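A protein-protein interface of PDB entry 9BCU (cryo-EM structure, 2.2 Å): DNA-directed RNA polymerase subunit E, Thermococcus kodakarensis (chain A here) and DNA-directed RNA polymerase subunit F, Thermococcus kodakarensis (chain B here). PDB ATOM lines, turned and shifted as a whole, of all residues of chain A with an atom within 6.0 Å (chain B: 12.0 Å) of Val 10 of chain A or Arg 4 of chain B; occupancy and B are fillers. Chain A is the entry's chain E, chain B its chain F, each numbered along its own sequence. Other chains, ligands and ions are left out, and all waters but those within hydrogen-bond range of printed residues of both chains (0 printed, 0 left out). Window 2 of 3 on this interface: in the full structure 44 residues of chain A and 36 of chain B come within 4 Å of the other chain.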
ATOM      1  N   VAL A   7      -1.155  28.895  -6.600  1.00  0.00           N
ATOM      2  CA  VAL A   7      -0.154  29.207  -7.612  1.00  0.00           C
ATOM      3  C   VAL A   7       0.046  27.988  -8.501  1.00  0.00           C
ATOM      4  O   VAL A   7       0.199  26.867  -8.003  1.00  0.00           O
ATOM      5  CB  VAL A   7       1.178  29.640  -6.971  1.00  0.00           C
ATOM      6  CG1 VAL A   7       2.211  29.947  -8.041  1.00  0.00           C
ATOM      7  CG2 VAL A   7       0.967  30.845  -6.069  1.00  0.00           C
ATOM      8  N   LYS A   8       0.040  28.210  -9.813  1.00  0.00           N
ATOM      9  CA  LYS A   8       0.366  27.183 -10.793  1.00  0.00           C
ATOM     10  C   LYS A   8       1.774  27.433 -11.320  1.00  0.00           C
ATOM     11  O   LYS A   8       2.094  28.549 -11.741  1.00  0.00           O
ATOM     12  CB  LYS A   8      -0.645  27.183 -11.942  1.00  0.00           C
ATOM     13  CG  LYS A   8      -0.117  26.598 -13.241  1.00  0.00           C
ATOM     14  CD  LYS A   8      -1.211  26.510 -14.292  1.00  0.00           C
ATOM     15  CE  LYS A   8      -2.264  25.484 -13.909  1.00  0.00           C
ATOM     16  NZ  LYS A   8      -1.946  24.134 -14.450  1.00  0.00           N
ATOM     17  N   ASP A   9       2.610  26.397 -11.290  1.00  0.00           N
ATOM     18  CA  ASP A   9       4.010  26.542 -11.662  1.00  0.00           C
ATOM     19  C   ASP A   9       4.510  25.242 -12.276  1.00  0.00           C
ATOM     20  O   ASP A   9       3.935  24.171 -12.070  1.00  0.00           O
ATOM     21  CB  ASP A   9       4.869  26.927 -10.450  1.00  0.00           C
ATOM     22  CG  ASP A   9       6.253  27.408 -10.840  1.00  0.00           C
ATOM     23  OD1 ASP A   9       6.470  27.697 -12.036  1.00  0.00           O
ATOM     24  OD2 ASP A   9       7.124  27.499  -9.950  1.00  0.00           O
ATOM     25  N   VAL A  10       5.594  25.355 -13.039  1.00  0.00           N
ATOM     26  CA  VAL A  10       6.277  24.199 -13.605  1.00  0.00           C
ATOM     27  C   VAL A  10       7.370  23.776 -12.632  1.00  0.00           C
ATOM     28  O   VAL A  10       8.226  24.584 -12.256  1.00  0.00           O
ATOM     29  CB  VAL A  10       6.860  24.518 -14.989  1.00  0.00           C
ATOM     30  CG1 VAL A  10       7.740  23.376 -15.472  1.00  0.00           C
ATOM     31  CG2 VAL A  10       5.743  24.794 -15.984  1.00  0.00           C
ATOM     32  N   VAL A  11       7.343  22.510 -12.222  1.00  0.00           N
ATOM     33  CA  VAL A  11       8.247  21.980 -11.209  1.00  0.00           C
ATOM     34  C   VAL A  11       9.178  20.971 -11.864  1.00  0.00           C
ATOM     35  O   VAL A  11       8.723  20.066 -12.575  1.00  0.00           O
ATOM     36  CB  VAL A  11       7.473  21.339 -10.045  1.00  0.00           C
ATOM     37  CG1 VAL A  11       8.425  20.921  -8.939  1.00  0.00           C
ATOM     38  CG2 VAL A  11       6.423  22.301  -9.514  1.00  0.00           C
ATOM     39  N   ARG A  12      10.477  21.124 -11.622  1.00  0.00           N
ATOM     40  CA  ARG A  12      11.487  20.193 -12.109  1.00  0.00           C
ATOM     41  C   ARG A  12      11.817  19.206 -10.998  1.00  0.00           C
ATOM     42  O   ARG A  12      12.211  19.610  -9.899  1.00  0.00           O
ATOM     43  CB  ARG A  12      12.746  20.935 -12.559  1.00  0.00           C
ATOM     44  CG  ARG A  12      13.914  20.020 -12.886  1.00  0.00           C
ATOM     45  CD  ARG A  12      15.244  20.728 -12.702  1.00  0.00           C
ATOM     46  NE  ARG A  12      16.352  19.954 -13.247  1.00  0.00           N
ATOM     47  CZ  ARG A  12      17.052  19.061 -12.558  1.00  0.00           C
ATOM     48  NH1 ARG A  12      16.787  18.806 -11.288  1.00  0.00           N
ATOM     49  NH2 ARG A  12      18.042  18.409 -13.162  1.00  0.00           N
ATOM     50  N   TYR A  34      11.114  27.855  -3.026  1.00  0.00           N
ATOM     51  CA  TYR A  34      10.415  29.084  -2.673  1.00  0.00           C
ATOM     52  C   TYR A  34      10.426  29.409  -1.185  1.00  0.00           C
ATOM     53  O   TYR A  34      10.273  30.581  -0.829  1.00  0.00           O
ATOM     54  CB  TYR A  34       8.958  29.017  -3.149  1.00  0.00           C
ATOM     55  CG  TYR A  34       8.790  29.236  -4.636  1.00  0.00           C
ATOM     56  CD1 TYR A  34       8.197  28.268  -5.436  1.00  0.00           C
ATOM     57  CD2 TYR A  34       9.224  30.409  -5.237  1.00  0.00           C
ATOM     58  CE1 TYR A  34       8.041  28.464  -6.795  1.00  0.00           C
ATOM     59  CE2 TYR A  34       9.072  30.614  -6.595  1.00  0.00           C
ATOM     60  CZ  TYR A  34       8.480  29.639  -7.369  1.00  0.00           C
ATOM     61  OH  TYR A  34       8.326  29.838  -8.720  1.00  0.00           O
ATOM     62  N   TYR A  67       9.537  17.628 -16.100  1.00  0.00           N
ATOM     63  CA  TYR A  67       8.903  18.891 -15.748  1.00  0.00           C
ATOM     64  C   TYR A  67       7.394  18.699 -15.712  1.00  0.00           C
ATOM     65  O   TYR A  67       6.801  18.211 -16.680  1.00  0.00           O
ATOM     66  CB  TYR A  67       9.281  19.990 -16.744  1.00  0.00           C
ATOM     67  CG  TYR A  67      10.731  20.413 -16.665  1.00  0.00           C
ATOM     68  CD1 TYR A  67      11.733  19.649 -17.252  1.00  0.00           C
ATOM     69  CD2 TYR A  67      11.100  21.578 -16.006  1.00  0.00           C
ATOM     70  CE1 TYR A  67      13.058  20.031 -17.182  1.00  0.00           C
ATOM     71  CE2 TYR A  67      12.424  21.970 -15.933  1.00  0.00           C
ATOM     72  CZ  TYR A  67      13.397  21.192 -16.522  1.00  0.00           C
ATOM     73  OH  TYR A  67      14.717  21.576 -16.451  1.00  0.00           O
ATOM     74  N   HIS A  68       6.778  19.088 -14.599  1.00  0.00           N
ATOM     75  CA  HIS A  68       5.354  18.890 -14.372  1.00  0.00           C
ATOM     76  C   HIS A  68       4.688  20.220 -14.055  1.00  0.00           C
ATOM     77  O   HIS A  68       5.282  21.082 -13.399  1.00  0.00           O
ATOM     78  CB  HIS A  68       5.103  17.910 -13.220  1.00  0.00           C
ATOM     79  CG  HIS A  68       5.682  16.548 -13.439  1.00  0.00           C
ATOM     80  ND1 HIS A  68       4.904  15.413 -13.520  1.00  0.00           N
ATOM     81  CD2 HIS A  68       6.964  16.133 -13.580  1.00  0.00           C
ATOM     82  CE1 HIS A  68       5.679  14.361 -13.708  1.00  0.00           C
ATOM     83  NE2 HIS A  68       6.934  14.771 -13.750  1.00  0.00           N
ATOM     84  N   GLU A  69       3.452  20.378 -14.517  1.00  0.00           N
ATOM     85  CA  GLU A  69       2.631  21.531 -14.165  1.00  0.00           C
ATOM     86  C   GLU A  69       1.882  21.216 -12.877  1.00  0.00           C
ATOM     87  O   GLU A  69       1.037  20.315 -12.850  1.00  0.00           O
ATOM     88  CB  GLU A  69       1.657  21.869 -15.292  1.00  0.00           C
ATOM     89  CG  GLU A  69       2.073  23.063 -16.135  1.00  0.00           C
ATOM     90  CD  GLU A  69       1.798  22.857 -17.612  1.00  0.00           C
ATOM     91  OE1 GLU A  69       0.919  22.034 -17.945  1.00  0.00           O
ATOM     92  OE2 GLU A  69       2.461  23.517 -18.439  1.00  0.00           O
ATOM     93  N   ALA A  70       2.189  21.954 -11.815  1.00  0.00           N
ATOM     94  CA  ALA A  70       1.659  21.675 -10.491  1.00  0.00           C
ATOM     95  C   ALA A  70       0.866  22.864  -9.968  1.00  0.00           C
ATOM     96  O   ALA A  70       1.186  24.023 -10.254  1.00  0.00           O
ATOM     97  CB  ALA A  70       2.780  21.328  -9.505  1.00  0.00           C
ATOM     98  N   MET B   1       7.457  37.496  -7.977  1.00  0.00           N
ATOM     99  CA  MET B   1       6.402  36.755  -8.659  1.00  0.00           C
ATOM    100  C   MET B   1       6.568  35.255  -8.437  1.00  0.00           C
ATOM    101  O   MET B   1       7.502  34.640  -8.954  1.00  0.00           O
ATOM    102  CB  MET B   1       6.402  37.077 -10.154  1.00  0.00           C
ATOM    103  CG  MET B   1       5.022  37.338 -10.734  1.00  0.00           C
ATOM    104  SD  MET B   1       4.130  35.825 -11.138  1.00  0.00           S
ATOM    105  CE  MET B   1       4.899  35.393 -12.697  1.00  0.00           C
ATOM    106  N   ILE B   2       5.659  34.673  -7.662  1.00  0.00           N
ATOM    107  CA  ILE B   2       5.731  33.254  -7.328  1.00  0.00           C
ATOM    108  C   ILE B   2       5.076  32.445  -8.440  1.00  0.00           C
ATOM    109  O   ILE B   2       3.915  32.680  -8.796  1.00  0.00           O
ATOM    110  CB  ILE B   2       5.060  32.979  -5.974  1.00  0.00           C
ATOM    111  CG1 ILE B   2       5.869  33.608  -4.839  1.00  0.00           C
ATOM    112  CG2 ILE B   2       4.903  31.482  -5.748  1.00  0.00           C
ATOM    113  CD1 ILE B   2       5.144  33.623  -3.512  1.00  0.00           C
ATOM    114  N   GLY B   3       5.823  31.492  -8.992  1.00  0.00           N
ATOM    115  CA  GLY B   3       5.276  30.608  -9.999  1.00  0.00           C
ATOM    116  C   GLY B   3       5.070  31.289 -11.343  1.00  0.00           C
ATOM    117  O   GLY B   3       5.612  32.361 -11.631  1.00  0.00           O
ATOM    118  N   ARG B   4       4.265  30.634 -12.180  1.00  0.00           N
ATOM    119  CA  ARG B   4       3.942  31.152 -13.503  1.00  0.00           C
ATOM    120  C   ARG B   4       2.757  32.109 -13.472  1.00  0.00           C
ATOM    121  O   ARG B   4       2.800  33.169 -14.106  1.00  0.00           O
ATOM    122  CB  ARG B   4       3.650  29.996 -14.463  1.00  0.00           C
ATOM    123  CG  ARG B   4       4.844  29.100 -14.742  1.00  0.00           C
ATOM    124  CD  ARG B   4       5.946  29.855 -15.466  1.00  0.00           C
ATOM    125  NE  ARG B   4       7.166  29.065 -15.578  1.00  0.00           N
ATOM    126  CZ  ARG B   4       7.396  28.173 -16.531  1.00  0.00           C
ATOM    127  NH1 ARG B   4       6.506  27.928 -17.478  1.00  0.00           N
ATOM    128  NH2 ARG B   4       8.549  27.510 -16.534  1.00  0.00           N
ATOM    129  N   LYS B   5       1.699  31.754 -12.747  1.00  0.00           N
ATOM    130  CA  LYS B   5       0.524  32.604 -12.636  1.00  0.00           C
ATOM    131  C   LYS B   5      -0.166  32.319 -11.311  1.00  0.00           C
ATOM    132  O   LYS B   5       0.048  31.278 -10.687  1.00  0.00           O
ATOM    133  CB  LYS B   5      -0.442  32.390 -13.807  1.00  0.00           C
ATOM    134  CG  LYS B   5      -1.317  31.154 -13.676  1.00  0.00           C
ATOM    135  CD  LYS B   5      -2.188  30.963 -14.907  1.00  0.00           C
ATOM    136  CE  LYS B   5      -3.579  31.538 -14.693  1.00  0.00           C
ATOM    137  NZ  LYS B   5      -4.580  30.920 -15.606  1.00  0.00           N
ATOM    138  N   LYS B   6      -1.000  33.265 -10.887  1.00  0.00           N
ATOM    139  CA  LYS B   6      -1.745  33.162  -9.640  1.00  0.00           C
ATOM    140  C   LYS B   6      -3.214  32.926  -9.964  1.00  0.00           C
ATOM    141  O   LYS B   6      -3.823  33.709 -10.701  1.00  0.00           O
ATOM    142  CB  LYS B   6      -1.573  34.424  -8.794  1.00  0.00           C
ATOM    143  CG  LYS B   6      -2.617  34.589  -7.703  1.00  0.00           C
ATOM    144  CD  LYS B   6      -2.056  35.350  -6.512  1.00  0.00           C
ATOM    145  CE  LYS B   6      -1.481  36.694  -6.933  1.00  0.00           C
ATOM    146  NZ  LYS B   6      -1.942  37.797  -6.046  1.00  0.00           N
ATOM    147  N   LEU B   7      -3.776  31.849  -9.416  1.00  0.00           N
ATOM    148  CA  LEU B   7      -5.173  31.520  -9.679  1.00  0.00           C
ATOM    149  C   LEU B   7      -6.109  32.335  -8.792  1.00  0.00           C
ATOM    150  O   LEU B   7      -6.958  33.082  -9.288  1.00  0.00           O
ATOM    151  CB  LEU B   7      -5.406  30.020  -9.477  1.00  0.00           C
ATOM    152  CG  LEU B   7      -4.462  29.080 -10.229  1.00  0.00           C
ATOM    153  CD1 LEU B   7      -4.836  27.628  -9.972  1.00  0.00           C
ATOM    154  CD2 LEU B   7      -4.473  29.383 -11.718  1.00  0.00           C
ATOM    155  N   GLU B   8      -5.965  32.202  -7.476  1.00  0.00           N
ATOM    156  CA  GLU B   8      -6.801  32.932  -6.538  1.00  0.00           C
ATOM    157  C   GLU B   8      -5.981  33.285  -5.307  1.00  0.00           C
ATOM    158  O   GLU B   8      -5.009  32.604  -4.973  1.00  0.00           O
ATOM    159  CB  GLU B   8      -8.038  32.121  -6.134  1.00  0.00           C
ATOM    160  CG  GLU B   8      -7.738  30.677  -5.771  1.00  0.00           C
ATOM    161  CD  GLU B   8      -8.806  30.065  -4.887  1.00  0.00           C
ATOM    162  OE1 GLU B   8      -8.961  30.523  -3.735  1.00  0.00           O
ATOM    163  OE2 GLU B   8      -9.491  29.125  -5.343  1.00  0.00           O
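Among the printed residues, pairs that only touch across the chains: Val 7 of chain A with Ile 2 of chain B (3.3 Å), Asp 9 of chain A with Gly 3 of chain B (3.4 Å), Val 10 of chain A with Arg 4 of chain B (3.6 Å), Val 7 of chain A with Lys 5 of chain B (3.7 Å) and Val 7 of chain A with Gly 3 of chain B (3.7 Å).
Of the printed residues of chain B, Val 7 of chain A touches Ile 2, Gly 3 and Lys 5. Of chain B, only Gly 3 and Arg 4 come within 4 Å of Asp 9 of chain A. Val 10 of chain A touches one residue of chain B. Val 11 of chain A touches none of the printed residues of chain B. No residue of chain B comes within 4 Å of Tyr 67 of chain A. No residue of chain B comes within 4 Å of Glu 69 of chain A. No residue of chain B comes within 4 Å of Ala 70 of chain A. Of the printed residues of chain A, Ile 2 of chain B touches Val 7 (3.3 Å). Of chain A, only Lys 8, Asp 9 and Val 10 come within 4 Å of Arg 4 of chain B. Leu 7 of chain B touches none of the printed residues of chain A. The nearest residue of chain B that does not touch Val 10 of chain A is Gly 3 of chain B (6.1 Å). The nearest residue of chain A that does not touch Arg 4 of chain B is Val 7 of chain A (4.7 Å). The nearest printed residue of chain A that does not touch Lys 5 of chain B is Asp 9 of chain A (5.5 Å).
Printed residues of chain A that touch a printed residue of chain B: Val 7, Lys 8, Asp 9, Val 10 and Tyr 34. Of the 8 printed residues of chain B, 4 touch a printed residue of chain A. Hydrophobic or aromatic side chains of chain B within 4 Å of the printed part of chain A: Ile 2. Among the printed residues, Asp or Glu carboxylates within 4 Å of a Lys or Arg side-chain nitrogen of the other chain: Asp 9 of chain A with Arg 4 of chain B.
The backbone carbonyl oxygen (O) of Lys 8 of chain A lies within hydrogen-bond range of the backbone NH (N) of Arg 4 of chain B (3.0 Å). The backbone NH of Lys 8 of chain A lies within hydrogen-bond range of the backbone carbonyl oxygen of Lys 5 of chain B (3.2 Å). OD1 of Asp 9 of chain A is in salt-bridge range of NE of Arg 4 of chain B, at 3.9 Å. The backbone NH (N) of Gly 3 of chain B sits at hydrogen-bond distance from the side-chain hydroxyl (OH) of Tyr 34 of chain A (3.0 Å).
The side-chain carboxylate of Asp 9 of chain A sits at hydrogen-bond distance from the side-chain hydroxyl of Tyr 34 of chain A (2.9 Å). The backbone NH (N) of Ala 70 of chain A is in hydrogen-bond range of the backbone carbonyl oxygen (O) of Asp 9 of chain A, 2.8 Å away.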
